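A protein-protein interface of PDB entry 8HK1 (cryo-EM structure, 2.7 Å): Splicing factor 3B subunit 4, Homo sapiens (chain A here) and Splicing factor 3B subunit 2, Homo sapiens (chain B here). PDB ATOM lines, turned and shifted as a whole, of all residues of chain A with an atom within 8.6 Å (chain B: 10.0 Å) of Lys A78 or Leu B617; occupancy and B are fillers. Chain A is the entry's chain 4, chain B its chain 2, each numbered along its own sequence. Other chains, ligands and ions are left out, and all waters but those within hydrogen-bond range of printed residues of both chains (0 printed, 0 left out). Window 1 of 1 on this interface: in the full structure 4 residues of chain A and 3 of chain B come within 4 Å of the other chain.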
ATOM      1  N   GLY A  19      26.649  30.786  28.906  1.00  0.00           N
ATOM      2  CA  GLY A  19      25.953  29.568  29.268  1.00  0.00           C
ATOM      3  C   GLY A  19      26.835  28.572  29.992  1.00  0.00           C
ATOM      4  O   GLY A  19      26.998  27.436  29.542  1.00  0.00           O
ATOM      5  N   LYS A  23      29.398  23.576  37.301  1.00  0.00           N
ATOM      6  CA  LYS A  23      30.478  22.605  37.149  1.00  0.00           C
ATOM      7  C   LYS A  23      31.656  23.192  36.382  1.00  0.00           C
ATOM      8  O   LYS A  23      32.800  22.763  36.584  1.00  0.00           O
ATOM      9  N   ILE A  73      33.548  26.175  16.535  1.00  0.00           N
ATOM     10  CA  ILE A  73      33.572  24.783  16.970  1.00  0.00           C
ATOM     11  C   ILE A  73      32.736  24.578  18.227  1.00  0.00           C
ATOM     12  O   ILE A  73      31.966  23.620  18.321  1.00  0.00           O
ATOM     13  N   MET A  74      32.873  25.470  19.208  1.00  0.00           N
ATOM     14  CA  MET A  74      32.174  25.350  20.479  1.00  0.00           C
ATOM     15  C   MET A  74      30.870  26.138  20.513  1.00  0.00           C
ATOM     16  O   MET A  74      30.455  26.585  21.589  1.00  0.00           O
ATOM     17  N   ASN A  75      30.217  26.319  19.367  1.00  0.00           N
ATOM     18  CA  ASN A  75      28.958  27.049  19.298  1.00  0.00           C
ATOM     19  C   ASN A  75      27.798  26.101  19.574  1.00  0.00           C
ATOM     20  O   ASN A  75      27.721  25.019  18.980  1.00  0.00           O
ATOM     21  N   MET A  76      26.902  26.524  20.482  1.00  0.00           N
ATOM     22  CA  MET A  76      25.691  25.788  20.877  1.00  0.00           C
ATOM     23  C   MET A  76      26.014  24.395  21.411  1.00  0.00           C
ATOM     24  O   MET A  76      25.313  23.421  21.127  1.00  0.00           O
ATOM     25  N   ILE A  77      27.086  24.296  22.195  1.00  0.00           N
ATOM     26  CA  ILE A  77      27.475  23.017  22.775  1.00  0.00           C
ATOM     27  C   ILE A  77      26.788  22.829  24.124  1.00  0.00           C
ATOM     28  O   ILE A  77      26.352  23.782  24.774  1.00  0.00           O
ATOM     29  N   LYS A  78      26.688  21.570  24.547  1.00  0.00           N
ATOM     30  CA  LYS A  78      26.064  21.213  25.819  1.00  0.00           C
ATOM     31  C   LYS A  78      27.180  20.941  26.823  1.00  0.00           C
ATOM     32  O   LYS A  78      27.658  19.813  26.963  1.00  0.00           O
ATOM     33  N   LEU A  79      27.597  21.989  27.530  1.00  0.00           N
ATOM     34  CA  LEU A  79      28.672  21.900  28.514  1.00  0.00           C
ATOM     35  C   LEU A  79      28.068  22.014  29.905  1.00  0.00           C
ATOM     36  O   LEU A  79      27.396  23.008  30.209  1.00  0.00           O
ATOM     37  N   TYR A  80      28.306  20.989  30.734  1.00  0.00           N
ATOM     38  CA  TYR A  80      27.824  20.893  32.120  1.00  0.00           C
ATOM     39  C   TYR A  80      26.305  21.007  32.216  1.00  0.00           C
ATOM     40  O   TYR A  80      25.773  21.562  33.182  1.00  0.00           O
ATOM     41  N   GLY A  81      25.596  20.474  31.225  1.00  0.00           N
ATOM     42  CA  GLY A  81      24.153  20.623  31.160  1.00  0.00           C
ATOM     43  C   GLY A  81      23.707  22.044  30.887  1.00  0.00           C
ATOM     44  O   GLY A  81      22.644  22.459  31.364  1.00  0.00           O
ATOM     45  N   LYS A  82      24.496  22.803  30.122  1.00  0.00           N
ATOM     46  CA  LYS A  82      24.205  24.204  29.869  1.00  0.00           C
ATOM     47  C   LYS A  82      24.551  24.543  28.425  1.00  0.00           C
ATOM     48  O   LYS A  82      25.537  24.014  27.893  1.00  0.00           O
ATOM     49  N   PRO A  83      23.763  25.407  27.769  1.00  0.00           N
ATOM     50  CA  PRO A  83      24.075  25.779  26.382  1.00  0.00           C
ATOM     51  C   PRO A  83      25.238  26.755  26.276  1.00  0.00           C
ATOM     52  O   PRO A  83      25.041  27.969  26.154  1.00  0.00           O
ATOM     53  CB  PRO A  83      22.765  26.401  25.887  1.00  0.00           C
ATOM     54  CG  PRO A  83      22.100  26.912  27.125  1.00  0.00           C
ATOM     55  CD  PRO A  83      22.476  25.961  28.221  1.00  0.00           C
ATOM     56  N   ILE A  84      26.462  26.228  26.311  1.00  0.00           N
ATOM     57  CA  ILE A  84      27.642  27.080  26.212  1.00  0.00           C
ATOM     58  C   ILE A  84      27.917  27.399  24.750  1.00  0.00           C
ATOM     59  O   ILE A  84      27.877  26.519  23.882  1.00  0.00           O
ATOM     60  N   ARG A  85      28.204  28.668  24.474  1.00  0.00           N
ATOM     61  CA  ARG A  85      28.488  29.113  23.117  1.00  0.00           C
ATOM     62  C   ARG A  85      29.510  30.237  23.165  1.00  0.00           C
ATOM     63  O   ARG A  85      29.452  31.098  24.047  1.00  0.00           O
ATOM     64  N   CYS A 168      16.922  25.883  22.223  1.00  0.00           N
ATOM     65  CA  CYS A 168      18.174  25.137  22.190  1.00  0.00           C
ATOM     66  C   CYS A 168      18.761  24.989  23.588  1.00  0.00           C
ATOM     67  O   CYS A 168      19.607  25.795  23.999  1.00  0.00           O
ATOM     68  N   ASN A 169      18.291  23.965  24.314  1.00  0.00           N
ATOM     69  CA  ASN A 169      18.758  23.592  25.659  1.00  0.00           C
ATOM     70  C   ASN A 169      18.586  24.732  26.668  1.00  0.00           C
ATOM     71  O   ASN A 169      19.393  24.901  27.583  1.00  0.00           O
ATOM     72  N   SER B 610      38.188  16.259  31.652  1.00  0.00           N
ATOM     73  CA  SER B 610      38.031  15.673  32.973  1.00  0.00           C
ATOM     74  C   SER B 610      36.802  14.774  33.022  1.00  0.00           C
ATOM     75  O   SER B 610      35.903  14.854  32.178  1.00  0.00           O
ATOM     76  N   ASP B 611      36.769  13.903  34.033  1.00  0.00           N
ATOM     77  CA  ASP B 611      35.645  12.985  34.183  1.00  0.00           C
ATOM     78  C   ASP B 611      34.409  13.690  34.723  1.00  0.00           C
ATOM     79  O   ASP B 611      33.283  13.330  34.354  1.00  0.00           O
ATOM     80  N   GLU B 612      34.594  14.696  35.586  1.00  0.00           N
ATOM     81  CA  GLU B 612      33.454  15.410  36.155  1.00  0.00           C
ATOM     82  C   GLU B 612      32.765  16.280  35.110  1.00  0.00           C
ATOM     83  O   GLU B 612      31.531  16.339  35.060  1.00  0.00           O
ATOM     84  N   LEU B 613      33.548  16.951  34.259  1.00  0.00           N
ATOM     85  CA  LEU B 613      32.964  17.757  33.191  1.00  0.00           C
ATOM     86  C   LEU B 613      32.295  16.892  32.133  1.00  0.00           C
ATOM     87  O   LEU B 613      31.262  17.283  31.574  1.00  0.00           O
ATOM     88  N   ARG B 614      32.852  15.710  31.853  1.00  0.00           N
ATOM     89  CA  ARG B 614      32.226  14.799  30.901  1.00  0.00           C
ATOM     90  C   ARG B 614      30.966  14.168  31.479  1.00  0.00           C
ATOM     91  O   ARG B 614      30.036  13.850  30.727  1.00  0.00           O
ATOM     92  N   ILE B 615      30.914  13.979  32.796  1.00  0.00           N
ATOM     93  CA  ILE B 615      29.703  13.454  33.417  1.00  0.00           C
ATOM     94  C   ILE B 615      28.623  14.532  33.505  1.00  0.00           C
ATOM     95  O   ILE B 615      27.432  14.232  33.370  1.00  0.00           O
ATOM     96  N   SER B 616      29.014  15.786  33.730  1.00  0.00           N
ATOM     97  CA  SER B 616      28.034  16.866  33.811  1.00  0.00           C
ATOM     98  C   SER B 616      27.540  17.302  32.437  1.00  0.00           C
ATOM     99  O   SER B 616      26.401  17.767  32.315  1.00  0.00           O
ATOM    100  N   LEU B 617      28.367  17.161  31.401  1.00  0.00           N
ATOM    101  CA  LEU B 617      27.976  17.567  30.057  1.00  0.00           C
ATOM    102  C   LEU B 617      27.045  16.568  29.378  1.00  0.00           C
ATOM    103  O   LEU B 617      26.446  16.906  28.352  1.00  0.00           O
ATOM    104  N   GLY B 618      26.910  15.360  29.915  1.00  0.00           N
ATOM    105  CA  GLY B 618      26.042  14.369  29.311  1.00  0.00           C
ATOM    106  C   GLY B 618      26.697  13.524  28.243  1.00  0.00           C
ATOM    107  O   GLY B 618      26.006  13.012  27.357  1.00  0.00           O
ATOM    108  N   MET B 619      28.021  13.361  28.299  1.00  0.00           N
ATOM    109  CA  MET B 619      28.740  12.563  27.315  1.00  0.00           C
ATOM    110  C   MET B 619      29.001  11.171  27.863  1.00  0.00           C
ATOM    111  O   MET B 619      29.508  11.042  28.990  1.00  0.00           O
ATOM    112  N   PRO B 620      28.676  10.115  27.121  1.00  0.00           N
ATOM    113  CA  PRO B 620      28.917   8.755  27.613  1.00  0.00           C
ATOM    114  C   PRO B 620      30.393   8.387  27.538  1.00  0.00           C
ATOM    115  O   PRO B 620      31.223   9.104  26.981  1.00  0.00           O
ATOM    116  CB  PRO B 620      28.082   7.889  26.665  1.00  0.00           C
ATOM    117  CG  PRO B 620      28.031   8.674  25.402  1.00  0.00           C
ATOM    118  CD  PRO B 620      27.999  10.120  25.813  1.00  0.00           C
ATOM    119  N   PRO B 630      32.774  13.711  20.533  1.00  0.00           N
ATOM    120  CA  PRO B 630      32.182  14.852  21.243  1.00  0.00           C
ATOM    121  C   PRO B 630      31.423  15.742  20.275  1.00  0.00           C
ATOM    122  O   PRO B 630      31.659  15.682  19.060  1.00  0.00           O
ATOM    123  CB  PRO B 630      33.411  15.568  21.832  1.00  0.00           C
ATOM    124  CG  PRO B 630      34.537  15.174  20.957  1.00  0.00           C
ATOM    125  CD  PRO B 630      34.247  13.767  20.526  1.00  0.00           C
ATOM    126  N   PRO B 631      30.488  16.570  20.763  1.00  0.00           N
ATOM    127  CA  PRO B 631      29.732  17.441  19.845  1.00  0.00           C
ATOM    128  C   PRO B 631      30.554  18.559  19.216  1.00  0.00           C
ATOM    129  O   PRO B 631      30.075  19.189  18.265  1.00  0.00           O
ATOM    130  CB  PRO B 631      28.618  18.009  20.736  1.00  0.00           C
ATOM    131  CG  PRO B 631      29.155  17.922  22.113  1.00  0.00           C
ATOM    132  CD  PRO B 631      29.987  16.677  22.147  1.00  0.00           C
ATOM    133  N   TRP B 632      31.761  18.830  19.712  1.00  0.00           N
ATOM    134  CA  TRP B 632      32.661  19.769  19.052  1.00  0.00           C
ATOM    135  C   TRP B 632      33.477  19.119  17.942  1.00  0.00           C
ATOM    136  O   TRP B 632      34.154  19.832  17.193  1.00  0.00           O
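Printed residues of chain B within 4 Å of Ile A73: Trp B632 (3.98 Å). No residue of chain B comes within 4 Å of Ile A77. Lys A78 touches one residue of chain B. No residue of chain B comes within 4 Å of Leu A79. Of chain B, only Ser B616 and Leu B617 come within 4 Å of Tyr A80. No residue of chain B comes within 4 Å of Lys A82. Leu B613 touches none of the printed residues of chain A. Leu B617 touches three residues of chain A. No residue of chain A comes within 4 Å of Gly B618. Of the printed residues of chain A, Trp B632 touches Ile A73 (3.98 Å). The nearest residue of chain A that does not touch Leu B617 is Leu A79 (4.5 Å). The nearest printed residue of chain B that does not touch Gly A81 is Gly B618 (5.4 Å).
O of Ser B616 is in hydrogen-bond range of N of Gly A81. O of Lys A78 sits close to O of Leu B617 (3.4 Å).
Among the printed residues, merely in contact across the chains: Ile A73 with Trp B632 (3.98 Å), Tyr A80 with Ser B616 (3.2 Å), Tyr A80 with Leu B617 (3.5 Å) and Gly A81 with Leu B617 (3.9 Å).
Along chain B the printed residues that touch a printed residue of chain A span positions 616 to 632. Of the 17 printed residues of chain A, 4 touch a printed residue of chain B. Among the printed residues, 6 pairs touch across the chains.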
